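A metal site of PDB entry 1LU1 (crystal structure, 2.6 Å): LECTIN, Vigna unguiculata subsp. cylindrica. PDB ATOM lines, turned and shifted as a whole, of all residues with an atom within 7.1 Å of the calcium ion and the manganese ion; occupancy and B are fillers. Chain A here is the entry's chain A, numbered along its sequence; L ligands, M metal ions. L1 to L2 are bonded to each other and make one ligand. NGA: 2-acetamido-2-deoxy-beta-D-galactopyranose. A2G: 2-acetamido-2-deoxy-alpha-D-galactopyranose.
The side-chain carboxylate of Asp 85 is in hydrogen-bond range of an oxygen (O4) of A2G L2, at 2.7 Å.
ND2 of Asn 129 is in hydrogen-bond range of O3 of A2G L2, 3.1 Å away.
N of Gly 103 lies within hydrogen-bond range of O7 of A2G L2, at 2.8 Å.
OD1 of Asp 133 sits close to NE1 of Trp 132, at 3.4 Å.
The side-chain carboxylate (OD2) of Asp 142 lies close to the side-chain carboxylate (OE1) of Glu 123, at 2.6 Å.
The backbone NH of Glu 123 lies within hydrogen-bond range of the backbone carbonyl oxygen of Gly 140, at 2.9 Å.
The side-chain carboxylate of Asp 142 is in hydrogen-bond range of the side-chain hydroxyl of Ser 148.
Within 4 Å of the calcium ion: Asp 125, Leu 127, Asn 129 and Asp 133.
The nearest printed residue that does not touch the calcium ion is Asp 85 (4.3 Å).
Residues that only touch the manganese ion: Ser 148 (3.5 Å).
The calcium ion is bound by OD1 of Asn 129, O of Leu 127, OD1 of Asp 125, OD2 of Asp 133 and OD2 of Asp 125.
The manganese ion is bound by OE2 of Glu 123, OD1 of Asp 133, OD2 of Asp 125 and NE2 of His 138.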
ATOM      1  N   ASP A  85      -2.180  -4.680  -0.154  1.00  0.00           N
ATOM      2  CA  ASP A  85      -2.017  -5.139  -1.526  1.00  0.00           C
ATOM      3  C   ASP A  85      -1.455  -4.068  -2.444  1.00  0.00           C
ATOM      4  O   ASP A  85      -0.924  -4.368  -3.501  1.00  0.00           O
ATOM      5  CB  ASP A  85      -3.367  -5.609  -2.083  1.00  0.00           C
ATOM      6  CG  ASP A  85      -3.441  -7.116  -2.236  1.00  0.00           C
ATOM      7  OD1 ASP A  85      -2.684  -7.656  -3.062  1.00  0.00           O
ATOM      8  OD2 ASP A  85      -4.260  -7.739  -1.523  1.00  0.00           O
ATOM      9  N   GLY A  86      -1.601  -2.799  -2.048  1.00  0.00           N
ATOM     10  CA  GLY A  86      -1.080  -1.718  -2.864  1.00  0.00           C
ATOM     11  C   GLY A  86      -2.031  -0.551  -3.007  1.00  0.00           C
ATOM     12  O   GLY A  86      -3.181  -0.615  -2.589  1.00  0.00           O
ATOM     13  N   GLY A 102      -8.834  -6.764  -2.768  1.00  0.00           N
ATOM     14  CA  GLY A 102      -7.623  -7.560  -2.823  1.00  0.00           C
ATOM     15  C   GLY A 102      -6.643  -7.114  -3.894  1.00  0.00           C
ATOM     16  O   GLY A 102      -6.364  -5.917  -4.037  1.00  0.00           O
ATOM     17  N   GLY A 103      -6.134  -8.073  -4.651  1.00  0.00           N
ATOM     18  CA  GLY A 103      -5.166  -7.781  -5.699  1.00  0.00           C
ATOM     19  C   GLY A 103      -5.670  -6.956  -6.858  1.00  0.00           C
ATOM     20  O   GLY A 103      -4.901  -6.654  -7.779  1.00  0.00           O
ATOM     21  N   TYR A 104      -6.943  -6.597  -6.844  1.00  0.00           N
ATOM     22  CA  TYR A 104      -7.504  -5.785  -7.927  1.00  0.00           C
ATOM     23  C   TYR A 104      -7.470  -4.307  -7.555  1.00  0.00           C
ATOM     24  O   TYR A 104      -7.884  -3.444  -8.329  1.00  0.00           O
ATOM     25  CB  TYR A 104      -8.935  -6.245  -8.244  1.00  0.00           C
ATOM     26  CG  TYR A 104      -8.956  -7.586  -8.935  1.00  0.00           C
ATOM     27  CD1 TYR A 104      -8.745  -7.678 -10.303  1.00  0.00           C
ATOM     28  CD2 TYR A 104      -9.133  -8.769  -8.206  1.00  0.00           C
ATOM     29  CE1 TYR A 104      -8.704  -8.907 -10.953  1.00  0.00           C
ATOM     30  CE2 TYR A 104      -9.104 -10.013  -8.847  1.00  0.00           C
ATOM     31  CZ  TYR A 104      -8.888 -10.077 -10.224  1.00  0.00           C
ATOM     32  OH  TYR A 104      -8.851 -11.292 -10.860  1.00  0.00           O
ATOM     33  N   LEU A 105      -6.966  -4.032  -6.354  1.00  0.00           N
ATOM     34  CA  LEU A 105      -6.813  -2.668  -5.850  1.00  0.00           C
ATOM     35  C   LEU A 105      -8.066  -1.805  -5.919  1.00  0.00           C
ATOM     36  O   LEU A 105      -7.990  -0.582  -5.856  1.00  0.00           O
ATOM     37  CB  LEU A 105      -5.676  -1.978  -6.602  1.00  0.00           C
ATOM     38  CG  LEU A 105      -4.344  -2.740  -6.655  1.00  0.00           C
ATOM     39  CD1 LEU A 105      -3.349  -2.005  -7.553  1.00  0.00           C
ATOM     40  CD2 LEU A 105      -3.789  -2.874  -5.231  1.00  0.00           C
ATOM     41  N   GLU A 123      -0.131   1.894 -10.677  1.00  0.00           N
ATOM     42  CA  GLU A 123      -0.161   1.178  -9.420  1.00  0.00           C
ATOM     43  C   GLU A 123       1.187   0.991  -8.778  1.00  0.00           C
ATOM     44  O   GLU A 123       2.224   0.905  -9.448  1.00  0.00           O
ATOM     45  CB  GLU A 123      -0.765  -0.201  -9.615  1.00  0.00           C
ATOM     46  CG  GLU A 123      -0.073  -0.960 -10.714  1.00  0.00           C
ATOM     47  CD  GLU A 123      -0.194  -2.451 -10.570  1.00  0.00           C
ATOM     48  OE1 GLU A 123      -1.241  -3.015 -10.961  1.00  0.00           O
ATOM     49  OE2 GLU A 123       0.760  -3.067 -10.053  1.00  0.00           O
ATOM     50  N   PHE A 124       1.136   0.908  -7.456  1.00  0.00           N
ATOM     51  CA  PHE A 124       2.297   0.669  -6.629  1.00  0.00           C
ATOM     52  C   PHE A 124       1.880  -0.593  -5.870  1.00  0.00           C
ATOM     53  O   PHE A 124       1.341  -0.568  -4.764  1.00  0.00           O
ATOM     54  CB  PHE A 124       2.531   1.887  -5.731  1.00  0.00           C
ATOM     55  CG  PHE A 124       2.700   3.159  -6.526  1.00  0.00           C
ATOM     56  CD1 PHE A 124       1.598   3.868  -6.988  1.00  0.00           C
ATOM     57  CD2 PHE A 124       3.974   3.628  -6.871  1.00  0.00           C
ATOM     58  CE1 PHE A 124       1.756   4.995  -7.782  1.00  0.00           C
ATOM     59  CE2 PHE A 124       4.144   4.771  -7.676  1.00  0.00           C
ATOM     60  CZ  PHE A 124       3.037   5.452  -8.128  1.00  0.00           C
ATOM     61  N   ASP A 125       2.125  -1.705  -6.567  1.00  0.00           N
ATOM     62  CA  ASP A 125       1.811  -3.062  -6.158  1.00  0.00           C
ATOM     63  C   ASP A 125       2.772  -3.647  -5.123  1.00  0.00           C
ATOM     64  O   ASP A 125       3.920  -3.915  -5.455  1.00  0.00           O
ATOM     65  CB  ASP A 125       1.834  -3.924  -7.405  1.00  0.00           C
ATOM     66  CG  ASP A 125       0.923  -5.105  -7.314  1.00  0.00           C
ATOM     67  OD1 ASP A 125       0.690  -5.578  -6.178  1.00  0.00           O
ATOM     68  OD2 ASP A 125       0.465  -5.569  -8.378  1.00  0.00           O
ATOM     69  N   THR A 126       2.310  -3.895  -3.906  1.00  0.00           N
ATOM     70  CA  THR A 126       3.176  -4.437  -2.869  1.00  0.00           C
ATOM     71  C   THR A 126       3.061  -5.953  -2.659  1.00  0.00           C
ATOM     72  O   THR A 126       3.659  -6.505  -1.740  1.00  0.00           O
ATOM     73  CB  THR A 126       2.920  -3.744  -1.523  1.00  0.00           C
ATOM     74  OG1 THR A 126       1.605  -4.057  -1.068  1.00  0.00           O
ATOM     75  CG2 THR A 126       3.035  -2.231  -1.689  1.00  0.00           C
ATOM     76  N   LEU A 127       2.289  -6.623  -3.506  1.00  0.00           N
ATOM     77  CA  LEU A 127       2.125  -8.077  -3.405  1.00  0.00           C
ATOM     78  C   LEU A 127       1.984  -8.689  -4.795  1.00  0.00           C
ATOM     79  O   LEU A 127       1.092  -8.327  -5.575  1.00  0.00           O
ATOM     80  CB  LEU A 127       0.907  -8.446  -2.563  1.00  0.00           C
ATOM     81  CG  LEU A 127       0.690  -9.956  -2.427  1.00  0.00           C
ATOM     82  CD1 LEU A 127       1.199 -10.427  -1.074  1.00  0.00           C
ATOM     83  CD2 LEU A 127      -0.768 -10.288  -2.592  1.00  0.00           C
ATOM     84  N   SER A 128       2.870  -9.633  -5.096  1.00  0.00           N
ATOM     85  CA  SER A 128       2.885 -10.294  -6.386  1.00  0.00           C
ATOM     86  C   SER A 128       1.803 -11.368  -6.518  1.00  0.00           C
ATOM     87  O   SER A 128       1.821 -12.366  -5.815  1.00  0.00           O
ATOM     88  CB  SER A 128       4.255 -10.924  -6.611  1.00  0.00           C
ATOM     89  OG  SER A 128       4.445 -11.206  -7.981  1.00  0.00           O
ATOM     90  N   ASN A 129       0.869 -11.156  -7.448  1.00  0.00           N
ATOM     91  CA  ASN A 129      -0.192 -12.122  -7.682  1.00  0.00           C
ATOM     92  C   ASN A 129       0.219 -13.000  -8.864  1.00  0.00           C
ATOM     93  O   ASN A 129       0.199 -12.562 -10.012  1.00  0.00           O
ATOM     94  CB  ASN A 129      -1.502 -11.409  -8.015  1.00  0.00           C
ATOM     95  CG  ASN A 129      -1.927 -10.443  -6.928  1.00  0.00           C
ATOM     96  OD1 ASN A 129      -1.722  -9.233  -7.050  1.00  0.00           O
ATOM     97  ND2 ASN A 129      -2.526 -10.968  -5.874  1.00  0.00           N
ATOM     98  N   TRP A 132      -0.702 -12.569 -12.847  1.00  0.00           N
ATOM     99  CA  TRP A 132      -0.425 -11.447 -13.752  1.00  0.00           C
ATOM    100  C   TRP A 132       0.678 -10.517 -13.272  1.00  0.00           C
ATOM    101  O   TRP A 132       1.021  -9.569 -13.966  1.00  0.00           O
ATOM    102  CB  TRP A 132      -1.689 -10.607 -13.926  1.00  0.00           C
ATOM    103  CG  TRP A 132      -2.175 -10.040 -12.615  1.00  0.00           C
ATOM    104  CD1 TRP A 132      -1.619  -9.010 -11.912  1.00  0.00           C
ATOM    105  CD2 TRP A 132      -3.297 -10.487 -11.855  1.00  0.00           C
ATOM    106  NE1 TRP A 132      -2.314  -8.792 -10.746  1.00  0.00           N
ATOM    107  CE2 TRP A 132      -3.364  -9.683 -10.690  1.00  0.00           C
ATOM    108  CE3 TRP A 132      -4.268 -11.487 -12.034  1.00  0.00           C
ATOM    109  CZ2 TRP A 132      -4.337  -9.852  -9.711  1.00  0.00           C
ATOM    110  CZ3 TRP A 132      -5.239 -11.662 -11.062  1.00  0.00           C
ATOM    111  CH2 TRP A 132      -5.275 -10.839  -9.919  1.00  0.00           C
ATOM    112  N   ASP A 133       1.234 -10.794 -12.103  1.00  0.00           N
ATOM    113  CA  ASP A 133       2.259  -9.921 -11.539  1.00  0.00           C
ATOM    114  C   ASP A 133       3.695 -10.370 -11.742  1.00  0.00           C
ATOM    115  O   ASP A 133       3.984 -11.565 -11.837  1.00  0.00           O
ATOM    116  CB  ASP A 133       2.020  -9.766 -10.031  1.00  0.00           C
ATOM    117  CG  ASP A 133       1.178  -8.557  -9.693  1.00  0.00           C
ATOM    118  OD1 ASP A 133       0.901  -7.768 -10.622  1.00  0.00           O
ATOM    119  OD2 ASP A 133       0.795  -8.402  -8.508  1.00  0.00           O
ATOM    120  N   PRO A 134       4.618  -9.404 -11.804  1.00  0.00           N
ATOM    121  CA  PRO A 134       6.048  -9.688 -11.976  1.00  0.00           C
ATOM    122  C   PRO A 134       6.564 -10.273 -10.670  1.00  0.00           C
ATOM    123  O   PRO A 134       5.868 -10.216  -9.664  1.00  0.00           O
ATOM    124  CB  PRO A 134       6.662  -8.310 -12.253  1.00  0.00           C
ATOM    125  CG  PRO A 134       5.501  -7.398 -12.516  1.00  0.00           C
ATOM    126  CD  PRO A 134       4.363  -7.959 -11.755  1.00  0.00           C
ATOM    127  N   HIS A 138       6.436  -3.784  -7.346  1.00  0.00           N
ATOM    128  CA  HIS A 138       6.644  -2.981  -8.535  1.00  0.00           C
ATOM    129  C   HIS A 138       5.696  -1.807  -8.751  1.00  0.00           C
ATOM    130  O   HIS A 138       4.667  -1.683  -8.099  1.00  0.00           O
ATOM    131  CB  HIS A 138       6.496  -3.894  -9.731  1.00  0.00           C
ATOM    132  CG  HIS A 138       5.186  -4.633  -9.757  1.00  0.00           C
ATOM    133  ND1 HIS A 138       4.884  -5.674  -8.915  1.00  0.00           N
ATOM    134  CD2 HIS A 138       4.061  -4.390 -10.469  1.00  0.00           C
ATOM    135  CE1 HIS A 138       3.608  -6.038  -9.138  1.00  0.00           C
ATOM    136  NE2 HIS A 138       3.060  -5.294 -10.076  1.00  0.00           N
ATOM    137  N   ILE A 139       6.075  -0.966  -9.709  1.00  0.00           N
ATOM    138  CA  ILE A 139       5.298   0.187 -10.104  1.00  0.00           C
ATOM    139  C   ILE A 139       4.857  -0.234 -11.499  1.00  0.00           C
ATOM    140  O   ILE A 139       5.654  -0.790 -12.245  1.00  0.00           O
ATOM    141  CB  ILE A 139       6.181   1.444 -10.228  1.00  0.00           C
ATOM    142  CG1 ILE A 139       6.798   1.771  -8.865  1.00  0.00           C
ATOM    143  CG2 ILE A 139       5.346   2.613 -10.735  1.00  0.00           C
ATOM    144  CD1 ILE A 139       7.931   2.775  -8.944  1.00  0.00           C
ATOM    145  N   GLY A 140       3.605   0.001 -11.859  1.00  0.00           N
ATOM    146  CA  GLY A 140       3.173  -0.422 -13.169  1.00  0.00           C
ATOM    147  C   GLY A 140       2.104   0.468 -13.754  1.00  0.00           C
ATOM    148  O   GLY A 140       1.416   1.176 -13.029  1.00  0.00           O
ATOM    149  N   ASP A 142      -1.351   0.452 -15.641  1.00  0.00           N
ATOM    150  CA  ASP A 142      -2.496  -0.391 -15.978  1.00  0.00           C
ATOM    151  C   ASP A 142      -3.500   0.299 -16.886  1.00  0.00           C
ATOM    152  O   ASP A 142      -4.026   1.352 -16.540  1.00  0.00           O
ATOM    153  CB  ASP A 142      -3.220  -0.838 -14.714  1.00  0.00           C
ATOM    154  CG  ASP A 142      -2.298  -1.491 -13.712  1.00  0.00           C
ATOM    155  OD1 ASP A 142      -1.261  -2.050 -14.132  1.00  0.00           O
ATOM    156  OD2 ASP A 142      -2.599  -1.430 -12.505  1.00  0.00           O
ATOM    157  N   ILE A 146      -5.829  -5.407 -14.785  1.00  0.00           N
ATOM    158  CA  ILE A 146      -4.921  -5.388 -13.642  1.00  0.00           C
ATOM    159  C   ILE A 146      -3.515  -5.881 -14.032  1.00  0.00           C
ATOM    160  O   ILE A 146      -2.578  -5.822 -13.229  1.00  0.00           O
ATOM    161  CB  ILE A 146      -5.480  -6.217 -12.461  1.00  0.00           C
ATOM    162  CG1 ILE A 146      -4.715  -5.874 -11.180  1.00  0.00           C
ATOM    163  CG2 ILE A 146      -5.397  -7.707 -12.762  1.00  0.00           C
ATOM    164  CD1 ILE A 146      -4.989  -4.467 -10.640  1.00  0.00           C
ATOM    165  N   LYS A 147      -3.383  -6.393 -15.258  1.00  0.00           N
ATOM    166  CA  LYS A 147      -2.085  -6.858 -15.742  1.00  0.00           C
ATOM    167  C   LYS A 147      -1.447  -5.627 -16.386  1.00  0.00           C
ATOM    168  O   LYS A 147      -1.856  -5.201 -17.469  1.00  0.00           O
ATOM    169  CB  LYS A 147      -2.269  -7.973 -16.785  1.00  0.00           C
ATOM    170  CG  LYS A 147      -1.049  -8.853 -16.954  1.00  0.00           C
ATOM    171  CD  LYS A 147      -0.861  -9.234 -18.428  1.00  0.00           C
ATOM    172  CE  LYS A 147      -0.568 -10.730 -18.599  1.00  0.00           C
ATOM    173  NZ  LYS A 147      -1.623 -11.571 -17.922  1.00  0.00           N
ATOM    174  N   SER A 148      -0.470  -5.049 -15.700  1.00  0.00           N
ATOM    175  CA  SER A 148       0.199  -3.853 -16.197  1.00  0.00           C
ATOM    176  C   SER A 148       0.818  -4.047 -17.579  1.00  0.00           C
ATOM    177  O   SER A 148       1.268  -5.144 -17.907  1.00  0.00           O
ATOM    178  CB  SER A 148       1.286  -3.440 -15.186  1.00  0.00           C
ATOM    179  OG  SER A 148       0.882  -3.705 -13.858  1.00  0.00           O
ATOM    180  N   THR A 151       6.124  -2.509 -16.271  1.00  0.00           N
ATOM    181  CA  THR A 151       6.414  -2.426 -14.838  1.00  0.00           C
ATOM    182  C   THR A 151       7.887  -2.172 -14.601  1.00  0.00           C
ATOM    183  O   THR A 151       8.676  -2.256 -15.531  1.00  0.00           O
ATOM    184  CB  THR A 151       6.067  -3.713 -14.093  1.00  0.00           C
ATOM    185  OG1 THR A 151       6.793  -4.799 -14.679  1.00  0.00           O
ATOM    186  CG2 THR A 151       4.576  -3.996 -14.174  1.00  0.00           C
HETATM  187  C1  NGA L   1      -3.682 -17.920  -2.185  1.00  0.00           C
HETATM  188  C2  NGA L   1      -3.536 -16.436  -2.493  1.00  0.00           C
HETATM  189  C3  NGA L   1      -4.834 -15.728  -2.221  1.00  0.00           C
HETATM  190  C4  NGA L   1      -6.053 -16.406  -2.832  1.00  0.00           C
HETATM  191  C5  NGA L   1      -6.046 -17.886  -2.512  1.00  0.00           C
HETATM  192  C6  NGA L   1      -7.185 -18.668  -3.186  1.00  0.00           C
HETATM  193  C7  NGA L   1      -1.492 -15.220  -2.275  1.00  0.00           C
HETATM  194  C8  NGA L   1      -0.429 -14.660  -1.359  1.00  0.00           C
HETATM  195  N2  NGA L   1      -2.483 -15.858  -1.678  1.00  0.00           N
HETATM  196  O1  NGA L   1      -2.546 -18.566  -2.650  1.00  0.00           O
HETATM  197  O3  NGA L   1      -4.751 -14.385  -2.749  1.00  0.00           O
HETATM  198  O4  NGA L   1      -6.024 -16.174  -4.235  1.00  0.00           O
HETATM  199  O5  NGA L   1      -4.781 -18.448  -2.920  1.00  0.00           O
HETATM  200  O7  NGA L   1      -1.454 -15.044  -3.518  1.00  0.00           O
HETATM  201  O5  A2G L   2      -5.002 -13.092  -0.693  1.00  0.00           O
HETATM  202  C1  A2G L   2      -5.462 -13.357  -2.040  1.00  0.00           C
HETATM  203  C2  A2G L   2      -5.508 -12.049  -2.858  1.00  0.00           C
HETATM  204  N2  A2G L   2      -5.825 -12.353  -4.240  1.00  0.00           N
HETATM  205  C3  A2G L   2      -4.179 -11.287  -2.793  1.00  0.00           C
HETATM  206  O3  A2G L   2      -4.296 -10.059  -3.506  1.00  0.00           O
HETATM  207  C4  A2G L   2      -3.813 -11.034  -1.325  1.00  0.00           C
HETATM  208  O4  A2G L   2      -4.842 -10.257  -0.729  1.00  0.00           O
HETATM  209  C5  A2G L   2      -3.743 -12.362  -0.605  1.00  0.00           C
HETATM  210  C6  A2G L   2      -3.427 -12.180   0.883  1.00  0.00           C
HETATM  211  O6  A2G L   2      -3.300 -13.444   1.495  1.00  0.00           O
HETATM  212  C7  A2G L   2      -6.699 -11.592  -4.916  1.00  0.00           C
HETATM  213  O7  A2G L   2      -7.286 -10.651  -4.395  1.00  0.00           O
HETATM  214  C8  A2G L   2      -6.969 -11.928  -6.379  1.00  0.00           C
HETATM  215 CA    CA M   1      -0.677  -7.413  -6.848  1.00  0.00          CA
HETATM  216 MN    MN M   2       0.638  -5.361 -10.806  1.00  0.00          MN
